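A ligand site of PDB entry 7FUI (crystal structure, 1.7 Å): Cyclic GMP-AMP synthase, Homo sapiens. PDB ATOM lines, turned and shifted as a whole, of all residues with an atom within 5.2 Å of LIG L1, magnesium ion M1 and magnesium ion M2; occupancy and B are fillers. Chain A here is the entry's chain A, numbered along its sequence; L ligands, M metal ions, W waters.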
ATOM      1  N   GLY A  52      21.438   4.009 -11.443  1.00  0.00           N
ATOM      2  CA  GLY A  52      21.343   2.568 -11.714  1.00  0.00           C
ATOM      3  C   GLY A  52      22.443   1.772 -11.034  1.00  0.00           C
ATOM      4  O   GLY A  52      23.209   2.342 -10.225  1.00  0.00           O
ATOM      5  N   SER A  53      22.515   0.485 -11.348  1.00  0.00           N
ATOM      6  CA  SER A  53      23.170  -0.543 -10.507  1.00  0.00           C
ATOM      7  C   SER A  53      24.689  -0.330 -10.471  1.00  0.00           C
ATOM      8  O   SER A  53      25.318  -0.635  -9.460  1.00  0.00           O
ATOM      9  CB  SER A  53      22.813  -1.922 -10.998  1.00  0.00           C
ATOM     10  OG  SER A  53      23.252  -2.109 -12.331  1.00  0.00           O
ATOM     11  N   TYR A  54      25.269   0.227 -11.527  1.00  0.00           N
ATOM     12  CA  TYR A  54      26.745   0.403 -11.515  1.00  0.00           C
ATOM     13  C   TYR A  54      27.149   1.380 -10.412  1.00  0.00           C
ATOM     14  O   TYR A  54      28.075   1.101  -9.650  1.00  0.00           O
ATOM     15  CB  TYR A  54      27.214   0.948 -12.847  1.00  0.00           C
ATOM     16  CG  TYR A  54      28.709   1.132 -12.857  1.00  0.00           C
ATOM     17  CD1 TYR A  54      29.572   0.064 -13.060  1.00  0.00           C
ATOM     18  CD2 TYR A  54      29.239   2.378 -12.576  1.00  0.00           C
ATOM     19  CE1 TYR A  54      30.947   0.255 -13.058  1.00  0.00           C
ATOM     20  CE2 TYR A  54      30.611   2.569 -12.545  1.00  0.00           C
ATOM     21  CZ  TYR A  54      31.463   1.510 -12.783  1.00  0.00           C
ATOM     22  OH  TYR A  54      32.813   1.777 -12.757  1.00  0.00           O
ATOM     23  N   GLU A  56      25.394   2.324  -7.852  1.00  0.00           N
ATOM     24  CA  GLU A  56      24.818   1.812  -6.585  1.00  0.00           C
ATOM     25  C   GLU A  56      25.664   0.639  -6.073  1.00  0.00           C
ATOM     26  O   GLU A  56      25.396   0.162  -4.939  1.00  0.00           O
ATOM     27  CB  GLU A  56      23.358   1.400  -6.782  1.00  0.00           C
ATOM     28  CG  GLU A  56      22.453   2.518  -7.219  1.00  0.00           C
ATOM     29  CD  GLU A  56      21.066   2.080  -7.684  1.00  0.00           C
ATOM     30  OE1 GLU A  56      20.918   0.917  -8.168  1.00  0.00           O
ATOM     31  OE2 GLU A  56      20.113   2.887  -7.482  1.00  0.00           O
ATOM     32  N   LYS A  59      25.589  -3.713  -9.489  1.00  0.00           N
ATOM     33  CA  LYS A  59      25.788  -4.350 -10.831  1.00  0.00           C
ATOM     34  C   LYS A  59      26.456  -5.708 -10.635  1.00  0.00           C
ATOM     35  O   LYS A  59      27.435  -5.766  -9.854  1.00  0.00           O
ATOM     36  CB  LYS A  59      26.662  -3.468 -11.718  1.00  0.00           C
ATOM     37  CG  LYS A  59      26.869  -3.988 -13.140  1.00  0.00           C
ATOM     38  CD  LYS A  59      25.699  -3.712 -14.047  1.00  0.00           C
ATOM     39  CE  LYS A  59      25.730  -4.466 -15.379  1.00  0.00           C
ATOM     40  NZ  LYS A  59      25.703  -5.939 -15.197  1.00  0.00           N
ATOM     41  N   GLU A  65      26.718  -2.495 -18.415  1.00  0.00           N
ATOM     42  CA  GLU A  65      25.445  -1.713 -18.526  1.00  0.00           C
ATOM     43  C   GLU A  65      25.459  -0.601 -17.485  1.00  0.00           C
ATOM     44  O   GLU A  65      25.554  -0.910 -16.239  1.00  0.00           O
ATOM     45  CB  GLU A  65      24.205  -2.608 -18.399  1.00  0.00           C
ATOM     46  CG  GLU A  65      22.957  -2.046 -19.093  1.00  0.00           C
ATOM     47  CD  GLU A  65      22.078  -1.172 -18.211  1.00  0.00           C
ATOM     48  OE1 GLU A  65      22.355  -1.131 -16.988  1.00  0.00           O
ATOM     49  OE2 GLU A  65      21.138  -0.552 -18.747  1.00  0.00           O
ATOM     50  N   PHE A  66      25.475   0.625 -17.983  1.00  0.00           N
ATOM     51  CA  PHE A  66      25.536   1.918 -17.236  1.00  0.00           C
ATOM     52  C   PHE A  66      24.264   2.721 -17.561  1.00  0.00           C
ATOM     53  O   PHE A  66      23.754   2.668 -18.701  1.00  0.00           O
ATOM     54  CB  PHE A  66      26.746   2.721 -17.671  1.00  0.00           C
ATOM     55  CG  PHE A  66      28.077   2.136 -17.286  1.00  0.00           C
ATOM     56  CD1 PHE A  66      28.564   1.012 -17.925  1.00  0.00           C
ATOM     57  CD2 PHE A  66      28.855   2.720 -16.300  1.00  0.00           C
ATOM     58  CE1 PHE A  66      29.787   0.476 -17.572  1.00  0.00           C
ATOM     59  CE2 PHE A  66      30.106   2.204 -15.970  1.00  0.00           C
ATOM     60  CZ  PHE A  66      30.562   1.089 -16.629  1.00  0.00           C
ATOM     61  N   ASP A  67      23.839   3.536 -16.624  1.00  0.00           N
ATOM     62  CA  ASP A  67      22.623   4.369 -16.727  1.00  0.00           C
ATOM     63  C   ASP A  67      22.988   5.777 -16.352  1.00  0.00           C
ATOM     64  O   ASP A  67      23.669   5.967 -15.320  1.00  0.00           O
ATOM     65  CB  ASP A  67      21.491   3.810 -15.863  1.00  0.00           C
ATOM     66  CG  ASP A  67      21.179   2.382 -16.201  1.00  0.00           C
ATOM     67  OD1 ASP A  67      20.465   2.178 -17.203  1.00  0.00           O
ATOM     68  OD2 ASP A  67      21.625   1.463 -15.442  1.00  0.00           O
ATOM     69  N   ASP A 159      22.531   3.475 -21.175  1.00  0.00           N
ATOM     70  CA  ASP A 159      21.171   4.044 -21.294  1.00  0.00           C
ATOM     71  C   ASP A 159      21.271   5.489 -20.843  1.00  0.00           C
ATOM     72  O   ASP A 159      21.769   5.737 -19.725  1.00  0.00           O
ATOM     73  CB  ASP A 159      20.124   3.290 -20.455  1.00  0.00           C
ATOM     74  CG  ASP A 159      19.779   1.880 -20.891  1.00  0.00           C
ATOM     75  OD1 ASP A 159      19.960   1.578 -22.088  1.00  0.00           O
ATOM     76  OD2 ASP A 159      19.351   1.083 -20.000  1.00  0.00           O
ATOM     77  N   ARG A 216       6.781  10.190 -17.050  1.00  0.00           N
ATOM     78  CA  ARG A 216       6.612   9.405 -15.812  1.00  0.00           C
ATOM     79  C   ARG A 216       7.574   9.885 -14.723  1.00  0.00           C
ATOM     80  O   ARG A 216       8.728  10.199 -15.055  1.00  0.00           O
ATOM     81  CB  ARG A 216       6.826   7.928 -16.102  1.00  0.00           C
ATOM     82  CG  ARG A 216       6.249   7.015 -15.022  1.00  0.00           C
ATOM     83  CD  ARG A 216       6.998   5.717 -14.850  1.00  0.00           C
ATOM     84  NE  ARG A 216       8.338   6.055 -14.390  1.00  0.00           N
ATOM     85  CZ  ARG A 216       9.487   5.585 -14.868  1.00  0.00           C
ATOM     86  NH1 ARG A 216      10.599   6.074 -14.398  1.00  0.00           N
ATOM     87  NH2 ARG A 216       9.525   4.642 -15.813  1.00  0.00           N
ATOM     88  N   LEU A 217       7.142   9.885 -13.463  1.00  0.00           N
ATOM     89  CA  LEU A 217       8.061  10.253 -12.348  1.00  0.00           C
ATOM     90  C   LEU A 217       9.265   9.303 -12.300  1.00  0.00           C
ATOM     91  O   LEU A 217       9.123   8.081 -12.596  1.00  0.00           O
ATOM     92  CB  LEU A 217       7.313  10.233 -11.025  1.00  0.00           C
ATOM     93  CG  LEU A 217       6.261  11.327 -10.861  1.00  0.00           C
ATOM     94  CD1 LEU A 217       5.487  11.090  -9.567  1.00  0.00           C
ATOM     95  CD2 LEU A 217       6.951  12.691 -10.842  1.00  0.00           C
ATOM     96  N   SER A 220      15.256   7.928  -9.399  1.00  0.00           N
ATOM     97  CA  SER A 220      16.532   7.167  -9.532  1.00  0.00           C
ATOM     98  C   SER A 220      17.627   7.769  -8.654  1.00  0.00           C
ATOM     99  O   SER A 220      18.436   7.011  -8.087  1.00  0.00           O
ATOM    100  CB  SER A 220      16.970   7.107 -10.962  1.00  0.00           C
ATOM    101  OG  SER A 220      15.955   6.508 -11.734  1.00  0.00           O
ATOM    102  N   GLU A 223      16.971   6.651  -5.096  1.00  0.00           N
ATOM    103  CA  GLU A 223      17.284   5.200  -5.004  1.00  0.00           C
ATOM    104  C   GLU A 223      18.800   5.060  -4.790  1.00  0.00           C
ATOM    105  O   GLU A 223      19.229   4.231  -3.962  1.00  0.00           O
ATOM    106  CB  GLU A 223      16.818   4.444  -6.248  1.00  0.00           C
ATOM    107  CG  GLU A 223      15.331   4.464  -6.475  1.00  0.00           C
ATOM    108  CD  GLU A 223      14.837   3.894  -7.796  1.00  0.00           C
ATOM    109  OE1 GLU A 223      15.635   3.271  -8.519  1.00  0.00           O
ATOM    110  OE2 GLU A 223      13.635   4.059  -8.096  1.00  0.00           O
ATOM    111  N   LYS A 254      18.861 -10.276  -7.992  1.00  0.00           N
ATOM    112  CA  LYS A 254      19.021  -9.841  -9.405  1.00  0.00           C
ATOM    113  C   LYS A 254      19.473 -11.052 -10.228  1.00  0.00           C
ATOM    114  O   LYS A 254      18.918 -11.264 -11.317  1.00  0.00           O
ATOM    115  CB  LYS A 254      20.037  -8.713  -9.508  1.00  0.00           C
ATOM    116  CG  LYS A 254      19.566  -7.376  -8.961  1.00  0.00           C
ATOM    117  CD  LYS A 254      20.702  -6.409  -8.711  1.00  0.00           C
ATOM    118  CE  LYS A 254      21.330  -5.824  -9.960  1.00  0.00           C
ATOM    119  NZ  LYS A 254      20.328  -5.341 -10.941  1.00  0.00           N
ATOM    120  N   GLU A 258      17.829 -12.860 -13.388  1.00  0.00           N
ATOM    121  CA  GLU A 258      18.582 -12.914 -14.673  1.00  0.00           C
ATOM    122  C   GLU A 258      18.667 -14.389 -15.120  1.00  0.00           C
ATOM    123  O   GLU A 258      18.448 -14.689 -16.303  1.00  0.00           O
ATOM    124  CB  GLU A 258      19.981 -12.299 -14.549  1.00  0.00           C
ATOM    125  CG  GLU A 258      20.022 -10.779 -14.368  1.00  0.00           C
ATOM    126  CD  GLU A 258      21.409 -10.123 -14.406  1.00  0.00           C
ATOM    127  OE1 GLU A 258      22.372 -10.876 -14.728  1.00  0.00           O
ATOM    128  OE2 GLU A 258      21.543  -8.837 -14.158  1.00  0.00           O
ATOM    129  N   SER A 275      14.772  -6.250 -13.569  1.00  0.00           N
ATOM    130  CA  SER A 275      15.566  -6.076 -12.335  1.00  0.00           C
ATOM    131  C   SER A 275      14.900  -5.031 -11.436  1.00  0.00           C
ATOM    132  O   SER A 275      15.069  -5.142 -10.213  1.00  0.00           O
ATOM    133  CB  SER A 275      17.011  -5.736 -12.662  1.00  0.00           C
ATOM    134  OG  SER A 275      17.134  -4.413 -13.175  1.00  0.00           O
ATOM    135  N   TYR A 276      14.135  -4.079 -11.986  1.00  0.00           N
ATOM    136  CA  TYR A 276      13.502  -3.000 -11.184  1.00  0.00           C
ATOM    137  C   TYR A 276      12.376  -3.594 -10.299  1.00  0.00           C
ATOM    138  O   TYR A 276      12.128  -3.016  -9.213  1.00  0.00           O
ATOM    139  CB  TYR A 276      12.926  -1.866 -12.044  1.00  0.00           C
ATOM    140  CG  TYR A 276      12.502  -0.657 -11.225  1.00  0.00           C
ATOM    141  CD1 TYR A 276      13.430   0.071 -10.502  1.00  0.00           C
ATOM    142  CD2 TYR A 276      11.172  -0.266 -11.110  1.00  0.00           C
ATOM    143  CE1 TYR A 276      13.062   1.184  -9.774  1.00  0.00           C
ATOM    144  CE2 TYR A 276      10.788   0.827 -10.330  1.00  0.00           C
ATOM    145  CZ  TYR A 276      11.739   1.548  -9.644  1.00  0.00           C
ATOM    146  OH  TYR A 276      11.424   2.649  -8.888  1.00  0.00           O
ATOM    147  N   LYS A 279      14.402  -4.809  -7.392  1.00  0.00           N
ATOM    148  CA  LYS A 279      14.954  -3.661  -6.627  1.00  0.00           C
ATOM    149  C   LYS A 279      13.854  -3.070  -5.736  1.00  0.00           C
ATOM    150  O   LYS A 279      14.124  -2.815  -4.561  1.00  0.00           O
ATOM    151  CB  LYS A 279      15.552  -2.631  -7.595  1.00  0.00           C
ATOM    152  CG  LYS A 279      16.296  -1.485  -6.942  1.00  0.00           C
ATOM    153  CD  LYS A 279      16.598  -0.336  -7.903  1.00  0.00           C
ATOM    154  CE  LYS A 279      17.677   0.623  -7.436  1.00  0.00           C
ATOM    155  NZ  LYS A 279      17.802   1.818  -8.311  1.00  0.00           N
ATOM    156  N   ASN A 322       5.221   0.618  -6.359  1.00  0.00           N
ATOM    157  CA  ASN A 322       6.353   1.537  -6.560  1.00  0.00           C
ATOM    158  C   ASN A 322       6.725   2.099  -5.185  1.00  0.00           C
ATOM    159  O   ASN A 322       5.834   2.448  -4.373  1.00  0.00           O
ATOM    160  CB  ASN A 322       6.004   2.572  -7.626  1.00  0.00           C
ATOM    161  CG  ASN A 322       7.097   3.588  -7.868  1.00  0.00           C
ATOM    162  OD1 ASN A 322       7.465   4.336  -6.956  1.00  0.00           O
ATOM    163  ND2 ASN A 322       7.603   3.617  -9.084  1.00  0.00           N
HETATM  164  P1  LIG L   1      20.639  -3.566 -13.902  1.00  0.00           P
HETATM  165  O1  LIG L   1      20.963  -2.552 -14.968  1.00  0.00           O
HETATM  166  O2  LIG L   1      19.603  -4.580 -14.327  1.00  0.00           O
HETATM  167  O3  LIG L   1      21.849  -4.155 -13.252  1.00  0.00           O
HETATM  168  P2  LIG L   1      19.465  -1.166 -12.882  1.00  0.00           P
HETATM  169  O4  LIG L   1      18.864  -0.721 -11.603  1.00  0.00           O
HETATM  170  O5  LIG L   1      20.591  -0.347 -13.459  1.00  0.00           O
HETATM  171  O6  LIG L   1      19.949  -2.669 -12.764  1.00  0.00           O
HETATM  172  P3  LIG L   1      18.033  -0.504 -15.360  1.00  0.00           P
HETATM  173  O7  LIG L   1      16.990  -1.269 -16.061  1.00  0.00           O
HETATM  174  O8  LIG L   1      19.344  -0.253 -16.062  1.00  0.00           O
HETATM  175  O9  LIG L   1      18.340  -1.279 -14.008  1.00  0.00           O
HETATM  176  O10 LIG L   1      17.391   0.870 -14.828  1.00  0.00           O
HETATM  177  C1  LIG L   1      18.187   1.991 -14.397  1.00  0.00           C
HETATM  178  C2  LIG L   1      17.398   2.735 -13.348  1.00  0.00           C
HETATM  179  O11 LIG L   1      16.206   3.257 -13.969  1.00  0.00           O
HETATM  180  C3  LIG L   1      16.861   1.932 -12.163  1.00  0.00           C
HETATM  181  O12 LIG L   1      17.843   1.667 -11.164  1.00  0.00           O
HETATM  182  C4  LIG L   1      15.716   2.848 -11.716  1.00  0.00           C
HETATM  183  O13 LIG L   1      16.155   3.981 -10.978  1.00  0.00           O
HETATM  184  C5  LIG L   1      15.132   3.283 -13.061  1.00  0.00           C
HETATM  185  N1  LIG L   1      14.043   2.428 -13.562  1.00  0.00           N
HETATM  186  C6  LIG L   1      14.123   1.310 -14.345  1.00  0.00           C
HETATM  187  N2  LIG L   1      12.958   0.775 -14.597  1.00  0.00           N
HETATM  188  C7  LIG L   1      12.040   1.596 -13.949  1.00  0.00           C
HETATM  189  C8  LIG L   1      10.625   1.557 -13.828  1.00  0.00           C
HETATM  190  N3  LIG L   1       9.845   0.626 -14.379  1.00  0.00           N
HETATM  191  N4  LIG L   1      10.038   2.515 -13.071  1.00  0.00           N
HETATM  192  C9  LIG L   1      10.813   3.444 -12.508  1.00  0.00           C
HETATM  193  N5  LIG L   1      12.146   3.596 -12.577  1.00  0.00           N
HETATM  194  C10 LIG L   1      12.698   2.608 -13.307  1.00  0.00           C
HETATM  195  C1  LG2 L   2      10.971   0.401 -18.400  1.00  0.00           C
HETATM  196  O1  LG2 L   2       9.720  -0.902 -20.293  1.00  0.00           O
HETATM  197  C2  LG2 L   2      12.366   0.305 -18.714  1.00  0.00           C
HETATM  198  C3  LG2 L   2      13.067  -0.801 -19.429  1.00  0.00           C
HETATM  199  C4  LG2 L   2      12.744  -1.202 -20.719  1.00  0.00           C
HETATM  200  C5  LG2 L   2      13.428  -2.249 -21.339  1.00  0.00           C
HETATM  201  C6  LG2 L   2      14.438  -2.923 -20.671  1.00  0.00           C
HETATM  202  C7  LG2 L   2      14.746  -2.506 -19.392  1.00  0.00           C
HETATM  203  C8  LG2 L   2      14.085  -1.479 -18.750  1.00  0.00           C
HETATM  204  C9  LG2 L   2      15.863   4.793 -16.519  1.00  0.00           C
HETATM  205  C10 LG2 L   2      17.001   5.587 -16.131  1.00  0.00           C
HETATM  206  C11 LG2 L   2      18.207   5.746 -16.752  1.00  0.00           C
HETATM  207  N1  LG2 L   2      14.163   7.222 -14.664  1.00  0.00           N
HETATM  208  C12 LG2 L   2      14.366   6.292 -15.318  1.00  0.00           C
HETATM  209  C13 LG2 L   2      14.576   5.102 -16.095  1.00  0.00           C
HETATM  210  C14 LG2 L   2      13.410   4.298 -16.419  1.00  0.00           C
HETATM  211  O2  LG2 L   2      12.280   4.618 -16.003  1.00  0.00           O
HETATM  212  N2  LG2 L   2      13.638   3.196 -17.175  1.00  0.00           N
HETATM  213  C15 LG2 L   2      12.713   2.253 -17.525  1.00  0.00           C
HETATM  214  N3  LG2 L   2      11.427   2.470 -17.231  1.00  0.00           N
HETATM  215  C16 LG2 L   2      10.575   1.518 -17.668  1.00  0.00           C
HETATM  216  S1  LG2 L   2       9.758  -0.807 -18.869  1.00  0.00           S
HETATM  217  C17 LG2 L   2      10.351  -2.326 -18.224  1.00  0.00           C
HETATM  218  O3  LG2 L   2       8.541  -0.468 -18.176  1.00  0.00           O
HETATM  219  F1  LG2 L   2      15.755  -3.149 -18.705  1.00  0.00           F
HETATM  220  N4  LG2 L   2      13.208   1.231 -18.231  1.00  0.00           N
HETATM  221  O4  LG2 L   2      16.092   3.691 -17.275  1.00  0.00           O
HETATM  222  O5  LG2 L   2      19.008   6.518 -15.991  1.00  0.00           O
HETATM  223  N5  LG2 L   2      18.333   6.816 -14.782  1.00  0.00           N
HETATM  224  C18 LG2 L   2      17.183   6.218 -14.881  1.00  0.00           C
HETATM  225  C19 LG2 L   2      18.756   5.345 -18.070  1.00  0.00           C
HETATM  226 MG    MG M   1      21.339  -0.539 -15.298  1.00  0.00          MG
HETATM  227 MG    MG M   2      19.543   0.581 -18.034  1.00  0.00          MG
HETATM  228  O   HOH W   1      19.919  -1.245  -9.095  1.00  0.00           O
HETATM  229  O   HOH W   2      18.288  -1.119 -18.713  1.00  0.00           O
HETATM  230  O   HOH W   3      16.796  -2.477 -11.087  1.00  0.00           O
HETATM  231  O   HOH W   4      19.723  -7.507 -12.687  1.00  0.00           O
HETATM  232  O   HOH W   5       7.756   2.395 -11.719  1.00  0.00           O
HETATM  233  O   HOH W   6      23.345  -0.589 -14.422  1.00  0.00           O
HETATM  234  O   HOH W   7      18.196  -4.510 -16.520  1.00  0.00           O
HETATM  235  O   HOH W   8      17.666   1.624 -17.884  1.00  0.00           O
HETATM  236  O   HOH W   9      15.079  -2.818 -14.729  1.00  0.00           O
HETATM  237  O   HOH W  10      12.180  -1.568 -15.760  1.00  0.00           O
HETATM  238  O   HOH W  11      23.524  -6.271 -13.265  1.00  0.00           O
HETATM  239  O   HOH W  12      21.499  -4.171 -17.249  1.00  0.00           O
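OE1 of Glu 223 is in hydrogen-bond range of O13 of LIG L1, 2.6 Å away. OG of Ser 220 is in hydrogen-bond range of O13 of LIG L1. N of Ser 53 lies close to O5 of LIG L1 (3.0 Å). The side-chain hydroxyl of Ser 53 lies within hydrogen-bond range of an oxygen (O3) of LIG L1 (2.6 Å). An oxygen (O2) of LIG L1 lies within hydrogen-bond range of the side-chain hydroxyl of Ser 275, at 2.7 Å. The side-chain amino group of Lys 279 is in hydrogen-bond range of an oxygen (O12) of LIG L1 (2.9 Å). The side-chain amino group (NZ) of Lys 254 lies within salt-bridge range of an oxygen (O3) of LIG L1, at 3.0 Å. N5 of LIG L1 lies close to NH1 of Arg 216, 3.4 Å away. NH1 of Arg 216 lies within hydrogen-bond range of O2 of LG2 L2.
An oxygen (O11) of LIG L1 sits close to an oxygen (O4) of LG2 L2.
The backbone NH (N) of Asp 159 sits at hydrogen-bond distance from the backbone carbonyl oxygen (O) of Phe 66 (2.9 Å). NZ of Lys 279 is in salt-bridge range of OE1 of Glu 223 (2.6 Å). The side-chain hydroxyl of Tyr 276 sits at hydrogen-bond distance from the side-chain carboxylate of Glu 223 (2.7 Å). The backbone NH (N) of Lys 59 sits at hydrogen-bond distance from the backbone carbonyl oxygen (O) of Ser 53 (3.1 Å). The side-chain amino group (NZ) of Lys 279 is in salt-bridge range of the side-chain carboxylate (OE2) of Glu 56 (2.7 Å).
Residues that only touch LIG L1: Tyr 276 (3.3 Å), Gly 52 (3.5 Å) and Lys 59 (3.96 Å). Of the 19 residues printed, 12 come within 4 Å of LIG L1. The nearest printed residue that does not touch LIG L1 is Asp 159 (4.2 Å).
Ser 53 touches magnesium ion M1 (OG to MG, 3.9 Å). Within 4 Å of magnesium ion M1: Ser 53, Glu 65 and Asp 67. The nearest printed residue that does not touch magnesium ion M1 is Gly 52 (4.7 Å).
Within 4 Å of magnesium ion M2: Glu 65, Asp 67 and Asp 159. The nearest printed residue that does not touch magnesium ion M2 is Phe 66 (4.7 Å).
Magnesium ion M1 is bound by O5 of LIG L1 (2.0 Å), OD2 of Asp 67 (2.0 Å), OE1 of Glu 65 (2.1 Å), O1 of LIG L1 (2.1 Å), O8 of LIG L1 (2.2 Å) and water W6 (2.2 Å).
Magnesium ion M2 is bound by OD1 of Asp 67, 2.0 Å away. OD2 of Asp 159 binds magnesium ion M2 (2.0 Å). Magnesium ion M2 is bound by OE2 of Glu 65. Magnesium ion M2 is bound by O8 of LIG L1 (2.2 Å). Water W8 binds magnesium ion M2 (2.2 Å). Water W2 is bound to magnesium ion M2, 2.2 Å away. Magnesium ion M2 has six donor atoms within binding distance.
Water W6 bridges the side-chain hydroxyl (OG) of Ser 53 (2.6 Å) and the backbone carbonyl oxygen (O) of Glu 65 (2.9 Å). Water W8 lies within hydrogen-bond range of an oxygen (O4) of LG2 L2 (2.7 Å) and an oxygen (O10) of LIG L1 (3.2 Å). Water W11 lies within hydrogen-bond range of an oxygen (O3) of LIG L1, the side-chain amino group of Lys 59 and the side-chain carboxylate of Glu 258. Water W1 bridges OE1 of Glu 56 (2.6 Å) and O4 of LIG L1 (2.8 Å). Water W9 lies within hydrogen-bond range of an oxygen (O7) of LIG L1 (2.8 Å), the side-chain hydroxyl of Ser 275 (3.0 Å) and the backbone NH of Tyr 276 (3.2 Å). Water W4 lies within hydrogen-bond range of the side-chain carboxylate of Glu 258 (2.7 Å), the side-chain amino group of Lys 254 (2.8 Å) and an oxygen (O2) of LIG L1 (3.4 Å).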
